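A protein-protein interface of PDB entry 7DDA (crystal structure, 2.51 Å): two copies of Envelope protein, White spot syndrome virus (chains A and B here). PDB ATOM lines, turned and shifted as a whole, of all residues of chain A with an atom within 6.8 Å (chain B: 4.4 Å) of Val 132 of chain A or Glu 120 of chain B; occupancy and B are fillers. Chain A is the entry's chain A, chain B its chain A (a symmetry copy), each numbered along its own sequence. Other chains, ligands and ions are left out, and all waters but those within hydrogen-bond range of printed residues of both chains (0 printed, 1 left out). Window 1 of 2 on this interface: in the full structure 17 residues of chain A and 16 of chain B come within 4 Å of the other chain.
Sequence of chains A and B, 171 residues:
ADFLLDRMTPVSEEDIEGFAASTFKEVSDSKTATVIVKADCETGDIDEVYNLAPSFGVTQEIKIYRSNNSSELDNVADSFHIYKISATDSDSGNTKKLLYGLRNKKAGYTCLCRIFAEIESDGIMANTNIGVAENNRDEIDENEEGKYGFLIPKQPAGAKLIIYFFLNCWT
Val 132 of chain A touches three residues of chain B.
Of the printed residues of chain B, Arg 137 of chain A touches Glu 120 (2.7 Å).
Of the printed residues of chain B, Ile 130 of chain A touches Ser 121 (3.8 Å).
Glu 134 of chain A touches none of the printed residues of chain B.
The nearest printed residue of chain B that does not touch Val 132 of chain A is Ile 119 of chain B (6.2 Å).
The nearest residue of chain A that does not touch Glu 120 of chain B is Ile 115 of chain A (4.5 Å).
O of Gly 131 of chain A is in hydrogen-bond range of N of Leu 151 of chain A (2.7 Å).
The backbone carbonyl oxygen (O) of Glu 118 of chain B sits at hydrogen-bond distance from the backbone NH (N) of Ile 162 of chain B (2.9 Å).
The backbone carbonyl oxygen (O) of Lys 160 of chain B is in hydrogen-bond range of the backbone NH (N) of Glu 120 of chain B, 2.8 Å away.
Of the 14 printed residues of chain A, 5 touch a printed residue of chain B.
Hydrophobic or aromatic side chains of chain A that line the printed part of chain B: Phe 116 and Val 132.
Of the 8 printed residues of chain B, 4 touch a printed residue of chain A.
Among the printed residues, 8 pairs touch across the chains.
Among the printed residues, Asp or Glu carboxylates within 4 Å of a Lys or Arg side-chain nitrogen of the other chain: Arg 137 of chain A with Glu 120 of chain B (2.7 Å).
Among the printed residues, pairs that only touch across the chains: Phe 116 of chain A with Glu 118 of chain B (3.6 Å), Ile 130 of chain A with Ser 121 of chain B (3.8 Å), Gly 131 of chain A with Ser 121 of chain B (3.2 Å), Gly 131 of chain A with Asp 122 of chain B (3.9 Å), Val 132 of chain A with Glu 120 of chain B (3.5 Å) and Val 132 of chain A with Asp 122 of chain B (3.4 Å).
No position is printed for both chains.
Of the 8 pairs that touch across the chains among the printed residues, none has its exchanged pair printed and touching as well.
N of Val 132 of chain A sits at hydrogen-bond distance from O of Ser 121 of chain B, at 2.7 Å.
NH2 of Arg 137 of chain A lies within salt-bridge range of OE2 of Glu 120 of chain B (2.7 Å).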
ATOM      1  N   LYS A  97      25.809 -28.300 -20.650  1.00  0.00           N
ATOM      2  CA  LYS A  97      26.380 -27.204 -19.870  1.00  0.00           C
ATOM      3  C   LYS A  97      27.017 -26.200 -20.825  1.00  0.00           C
ATOM      4  O   LYS A  97      27.955 -26.544 -21.552  1.00  0.00           O
ATOM      5  CB  LYS A  97      27.391 -27.717 -18.854  1.00  0.00           C
ATOM      6  CG  LYS A  97      28.097 -26.630 -18.104  1.00  0.00           C
ATOM      7  CD  LYS A  97      27.157 -25.814 -17.247  1.00  0.00           C
ATOM      8  CE  LYS A  97      27.880 -24.595 -16.650  1.00  0.00           C
ATOM      9  NZ  LYS A  97      29.232 -24.908 -16.076  1.00  0.00           N
ATOM     10  N   ILE A 115      22.167 -11.114 -15.417  1.00  0.00           N
ATOM     11  CA  ILE A 115      21.758 -11.901 -16.572  1.00  0.00           C
ATOM     12  C   ILE A 115      20.354 -12.470 -16.418  1.00  0.00           C
ATOM     13  O   ILE A 115      19.839 -12.693 -15.318  1.00  0.00           O
ATOM     14  CB  ILE A 115      22.716 -13.071 -16.865  1.00  0.00           C
ATOM     15  CG1 ILE A 115      22.583 -14.097 -15.753  1.00  0.00           C
ATOM     16  CG2 ILE A 115      24.158 -12.588 -17.097  1.00  0.00           C
ATOM     17  CD1 ILE A 115      23.290 -15.353 -16.012  1.00  0.00           C
ATOM     18  N   PHE A 116      19.757 -12.732 -17.573  1.00  0.00           N
ATOM     19  CA  PHE A 116      18.545 -13.508 -17.718  1.00  0.00           C
ATOM     20  C   PHE A 116      18.710 -14.365 -18.972  1.00  0.00           C
ATOM     21  O   PHE A 116      19.283 -13.913 -19.972  1.00  0.00           O
ATOM     22  CB  PHE A 116      17.315 -12.593 -17.825  1.00  0.00           C
ATOM     23  CG  PHE A 116      16.055 -13.327 -18.187  1.00  0.00           C
ATOM     24  CD1 PHE A 116      15.522 -14.275 -17.326  1.00  0.00           C
ATOM     25  CD2 PHE A 116      15.445 -13.124 -19.420  1.00  0.00           C
ATOM     26  CE1 PHE A 116      14.378 -14.975 -17.668  1.00  0.00           C
ATOM     27  CE2 PHE A 116      14.298 -13.818 -19.763  1.00  0.00           C
ATOM     28  CZ  PHE A 116      13.759 -14.745 -18.883  1.00  0.00           C
ATOM     29  N   ILE A 130      16.210 -23.532 -16.863  1.00  0.00           N
ATOM     30  CA  ILE A 130      17.634 -23.273 -16.983  1.00  0.00           C
ATOM     31  C   ILE A 130      18.226 -23.204 -15.588  1.00  0.00           C
ATOM     32  O   ILE A 130      17.755 -22.433 -14.750  1.00  0.00           O
ATOM     33  CB  ILE A 130      17.898 -21.962 -17.737  1.00  0.00           C
ATOM     34  CG1 ILE A 130      17.258 -22.030 -19.120  1.00  0.00           C
ATOM     35  CG2 ILE A 130      19.400 -21.699 -17.800  1.00  0.00           C
ATOM     36  CD1 ILE A 130      17.384 -20.790 -19.880  1.00  0.00           C
ATOM     37  N   GLY A 131      19.263 -24.003 -15.340  1.00  0.00           N
ATOM     38  CA  GLY A 131      19.996 -23.921 -14.089  1.00  0.00           C
ATOM     39  C   GLY A 131      21.162 -22.960 -14.235  1.00  0.00           C
ATOM     40  O   GLY A 131      21.909 -23.020 -15.216  1.00  0.00           O
ATOM     41  N   VAL A 132      21.302 -22.066 -13.262  1.00  0.00           N
ATOM     42  CA  VAL A 132      22.414 -21.117 -13.227  1.00  0.00           C
ATOM     43  C   VAL A 132      23.612 -21.785 -12.577  1.00  0.00           C
ATOM     44  O   VAL A 132      23.482 -22.438 -11.537  1.00  0.00           O
ATOM     45  CB  VAL A 132      22.019 -19.837 -12.472  1.00  0.00           C
ATOM     46  CG1 VAL A 132      23.146 -18.794 -12.543  1.00  0.00           C
ATOM     47  CG2 VAL A 132      20.741 -19.262 -13.049  1.00  0.00           C
ATOM     48  N   ALA A 133      24.781 -21.638 -13.192  1.00  0.00           N
ATOM     49  CA  ALA A 133      26.010 -22.189 -12.629  1.00  0.00           C
ATOM     50  C   ALA A 133      26.964 -21.041 -12.337  1.00  0.00           C
ATOM     51  O   ALA A 133      26.720 -20.262 -11.411  1.00  0.00           O
ATOM     52  CB  ALA A 133      26.642 -23.219 -13.574  1.00  0.00           C
ATOM     53  N   GLU A 134      28.035 -20.915 -13.123  1.00  0.00           N
ATOM     54  CA  GLU A 134      28.908 -19.751 -13.013  1.00  0.00           C
ATOM     55  C   GLU A 134      28.111 -18.466 -13.202  1.00  0.00           C
ATOM     56  O   GLU A 134      27.301 -18.346 -14.128  1.00  0.00           O
ATOM     57  CB  GLU A 134      30.019 -19.808 -14.055  1.00  0.00           C
ATOM     58  CG  GLU A 134      31.065 -20.879 -13.828  1.00  0.00           C
ATOM     59  CD  GLU A 134      30.706 -22.207 -14.459  1.00  0.00           C
ATOM     60  OE1 GLU A 134      29.516 -22.448 -14.745  1.00  0.00           O
ATOM     61  OE2 GLU A 134      31.631 -23.007 -14.698  1.00  0.00           O
ATOM     62  N   ASN A 135      28.359 -17.498 -12.325  1.00  0.00           N
ATOM     63  CA  ASN A 135      27.699 -16.202 -12.412  1.00  0.00           C
ATOM     64  C   ASN A 135      28.551 -15.187 -11.665  1.00  0.00           C
ATOM     65  O   ASN A 135      28.593 -15.212 -10.437  1.00  0.00           O
ATOM     66  CB  ASN A 135      26.300 -16.277 -11.815  1.00  0.00           C
ATOM     67  CG  ASN A 135      25.480 -15.060 -12.128  1.00  0.00           C
ATOM     68  OD1 ASN A 135      26.005 -13.955 -12.238  1.00  0.00           O
ATOM     69  ND2 ASN A 135      24.177 -15.247 -12.261  1.00  0.00           N
ATOM     70  N   ARG A 137      28.921 -11.879 -10.066  1.00  0.00           N
ATOM     71  CA  ARG A 137      28.136 -10.772  -9.538  1.00  0.00           C
ATOM     72  C   ARG A 137      28.989  -9.585  -9.126  1.00  0.00           C
ATOM     73  O   ARG A 137      28.443  -8.567  -8.692  1.00  0.00           O
ATOM     74  CB  ARG A 137      27.311 -11.247  -8.334  1.00  0.00           C
ATOM     75  CG  ARG A 137      26.277 -12.246  -8.735  1.00  0.00           C
ATOM     76  CD  ARG A 137      25.876 -13.162  -7.622  1.00  0.00           C
ATOM     77  NE  ARG A 137      24.796 -14.046  -8.068  1.00  0.00           N
ATOM     78  CZ  ARG A 137      23.582 -13.648  -8.452  1.00  0.00           C
ATOM     79  NH1 ARG A 137      23.224 -12.364  -8.403  1.00  0.00           N
ATOM     80  NH2 ARG A 137      22.708 -14.555  -8.861  1.00  0.00           N
ATOM     81  N   TYR A 148      29.520 -16.775 -17.254  1.00  0.00           N
ATOM     82  CA  TYR A 148      28.112 -17.079 -17.018  1.00  0.00           C
ATOM     83  C   TYR A 148      27.789 -18.453 -17.585  1.00  0.00           C
ATOM     84  O   TYR A 148      27.905 -18.675 -18.792  1.00  0.00           O
ATOM     85  CB  TYR A 148      27.242 -15.973 -17.622  1.00  0.00           C
ATOM     86  CG  TYR A 148      27.640 -14.664 -16.961  1.00  0.00           C
ATOM     87  CD1 TYR A 148      27.221 -14.371 -15.665  1.00  0.00           C
ATOM     88  CD2 TYR A 148      28.510 -13.780 -17.581  1.00  0.00           C
ATOM     89  CE1 TYR A 148      27.626 -13.225 -15.021  1.00  0.00           C
ATOM     90  CE2 TYR A 148      28.924 -12.615 -16.936  1.00  0.00           C
ATOM     91  CZ  TYR A 148      28.477 -12.351 -15.662  1.00  0.00           C
ATOM     92  OH  TYR A 148      28.868 -11.203 -15.019  1.00  0.00           O
ATOM     93  N   GLY A 149      27.415 -19.382 -16.711  1.00  0.00           N
ATOM     94  CA  GLY A 149      27.213 -20.774 -17.086  1.00  0.00           C
ATOM     95  C   GLY A 149      25.764 -21.206 -16.915  1.00  0.00           C
ATOM     96  O   GLY A 149      25.116 -20.868 -15.921  1.00  0.00           O
ATOM     97  N   PHE A 150      25.277 -21.977 -17.878  1.00  0.00           N
ATOM     98  CA  PHE A 150      23.890 -22.399 -17.880  1.00  0.00           C
ATOM     99  C   PHE A 150      23.815 -23.910 -18.019  1.00  0.00           C
ATOM    100  O   PHE A 150      24.500 -24.492 -18.866  1.00  0.00           O
ATOM    101  CB  PHE A 150      23.143 -21.687 -18.996  1.00  0.00           C
ATOM    102  CG  PHE A 150      23.272 -20.195 -18.919  1.00  0.00           C
ATOM    103  CD1 PHE A 150      22.455 -19.460 -18.066  1.00  0.00           C
ATOM    104  CD2 PHE A 150      24.250 -19.531 -19.645  1.00  0.00           C
ATOM    105  CE1 PHE A 150      22.582 -18.085 -17.973  1.00  0.00           C
ATOM    106  CE2 PHE A 150      24.389 -18.149 -19.557  1.00  0.00           C
ATOM    107  CZ  PHE A 150      23.551 -17.426 -18.725  1.00  0.00           C
ATOM    108  N   LEU A 151      23.021 -24.542 -17.162  1.00  0.00           N
ATOM    109  CA  LEU A 151      22.686 -25.954 -17.301  1.00  0.00           C
ATOM    110  C   LEU A 151      21.337 -26.030 -17.992  1.00  0.00           C
ATOM    111  O   LEU A 151      20.341 -25.526 -17.461  1.00  0.00           O
ATOM    112  CB  LEU A 151      22.611 -26.642 -15.941  1.00  0.00           C
ATOM    113  CG  LEU A 151      22.353 -28.150 -15.896  1.00  0.00           C
ATOM    114  CD1 LEU A 151      23.371 -28.979 -16.691  1.00  0.00           C
ATOM    115  CD2 LEU A 151      22.276 -28.602 -14.449  1.00  0.00           C
ATOM    116  N   GLU B 118      11.065 -14.241 -12.329  1.00  0.00           N
ATOM    117  CA  GLU B 118      11.562 -15.556 -12.717  1.00  0.00           C
ATOM    118  C   GLU B 118      12.391 -16.149 -11.584  1.00  0.00           C
ATOM    119  O   GLU B 118      13.056 -15.429 -10.836  1.00  0.00           O
ATOM    120  CB  GLU B 118      12.334 -15.474 -14.053  1.00  0.00           C
ATOM    121  CG  GLU B 118      13.498 -14.439 -14.166  1.00  0.00           C
ATOM    122  CD  GLU B 118      14.901 -14.942 -13.864  1.00  0.00           C
ATOM    123  OE1 GLU B 118      15.106 -16.159 -13.858  1.00  0.00           O
ATOM    124  OE2 GLU B 118      15.828 -14.103 -13.753  1.00  0.00           O
ATOM    125  N   ILE B 119      12.284 -17.468 -11.425  1.00  0.00           N
ATOM    126  CA  ILE B 119      13.046 -18.192 -10.414  1.00  0.00           C
ATOM    127  C   ILE B 119      14.461 -18.442 -10.929  1.00  0.00           C
ATOM    128  O   ILE B 119      14.659 -18.947 -12.037  1.00  0.00           O
ATOM    129  CB  ILE B 119      12.349 -19.512 -10.056  1.00  0.00           C
ATOM    130  CG1 ILE B 119      10.908 -19.256  -9.625  1.00  0.00           C
ATOM    131  CG2 ILE B 119      13.131 -20.264  -8.971  1.00  0.00           C
ATOM    132  CD1 ILE B 119      10.776 -18.869  -8.196  1.00  0.00           C
ATOM    133  N   GLU B 120      15.448 -18.090 -10.128  1.00  0.00           N
ATOM    134  CA  GLU B 120      16.847 -18.316 -10.449  1.00  0.00           C
ATOM    135  C   GLU B 120      17.366 -19.412  -9.539  1.00  0.00           C
ATOM    136  O   GLU B 120      17.396 -19.255  -8.318  1.00  0.00           O
ATOM    137  CB  GLU B 120      17.666 -17.044 -10.279  1.00  0.00           C
ATOM    138  CG  GLU B 120      18.989 -17.091 -10.938  1.00  0.00           C
ATOM    139  CD  GLU B 120      19.791 -15.867 -10.628  1.00  0.00           C
ATOM    140  OE1 GLU B 120      19.724 -14.903 -11.418  1.00  0.00           O
ATOM    141  OE2 GLU B 120      20.469 -15.866  -9.574  1.00  0.00           O
ATOM    142  N   SER B 121      17.794 -20.500 -10.141  1.00  0.00           N
ATOM    143  CA  SER B 121      18.010 -21.759  -9.462  1.00  0.00           C
ATOM    144  C   SER B 121      19.155 -22.477 -10.150  1.00  0.00           C
ATOM    145  O   SER B 121      19.374 -22.317 -11.358  1.00  0.00           O
ATOM    146  CB  SER B 121      16.742 -22.615  -9.498  1.00  0.00           C
ATOM    147  OG  SER B 121      17.021 -23.937  -9.087  1.00  0.00           O
ATOM    148  N   ASP B 122      19.884 -23.269  -9.379  1.00  0.00           N
ATOM    149  CA  ASP B 122      20.967 -24.034  -9.963  1.00  0.00           C
ATOM    150  C   ASP B 122      20.508 -25.401 -10.455  1.00  0.00           C
ATOM    151  O   ASP B 122      21.271 -26.093 -11.131  1.00  0.00           O
ATOM    152  CB  ASP B 122      22.122 -24.121  -8.960  1.00  0.00           C
ATOM    153  CG  ASP B 122      21.861 -25.067  -7.846  1.00  0.00           C
ATOM    154  OD1 ASP B 122      20.704 -25.481  -7.667  1.00  0.00           O
ATOM    155  OD2 ASP B 122      22.808 -25.353  -7.091  1.00  0.00           O
ATOM    156  N   ALA B 159      17.397 -21.093  -3.869  1.00  0.00           N
ATOM    157  CA  ALA B 159      16.758 -20.542  -5.052  1.00  0.00           C
ATOM    158  C   ALA B 159      16.287 -19.111  -4.796  1.00  0.00           C
ATOM    159  O   ALA B 159      15.879 -18.758  -3.686  1.00  0.00           O
ATOM    160  CB  ALA B 159      15.582 -21.427  -5.471  1.00  0.00           C
ATOM    161  N   LYS B 160      16.338 -18.286  -5.843  1.00  0.00           N
ATOM    162  CA  LYS B 160      16.028 -16.867  -5.733  1.00  0.00           C
ATOM    163  C   LYS B 160      14.869 -16.474  -6.639  1.00  0.00           C
ATOM    164  O   LYS B 160      14.625 -17.087  -7.687  1.00  0.00           O
ATOM    165  CB  LYS B 160      17.245 -15.992  -6.080  1.00  0.00           C
ATOM    166  CG  LYS B 160      18.507 -16.265  -5.244  1.00  0.00           C
ATOM    167  CD  LYS B 160      18.236 -16.100  -3.757  1.00  0.00           C
ATOM    168  CE  LYS B 160      19.497 -16.259  -2.921  1.00  0.00           C
ATOM    169  NZ  LYS B 160      19.210 -15.984  -1.491  1.00  0.00           N
ATOM    170  N   ILE B 162      13.802 -13.353  -8.909  1.00  0.00           N
ATOM    171  CA  ILE B 162      14.297 -12.146  -9.561  1.00  0.00           C
ATOM    172  C   ILE B 162      13.089 -11.409 -10.124  1.00  0.00           C
ATOM    173  O   ILE B 162      12.363 -11.950 -10.969  1.00  0.00           O
ATOM    174  CB  ILE B 162      15.325 -12.461 -10.657  1.00  0.00           C
ATOM    175  CG1 ILE B 162      16.370 -13.468 -10.154  1.00  0.00           C
ATOM    176  CG2 ILE B 162      16.019 -11.208 -11.092  1.00  0.00           C
ATOM    177  CD1 ILE B 162      17.220 -12.977  -8.985  1.00  0.00           C
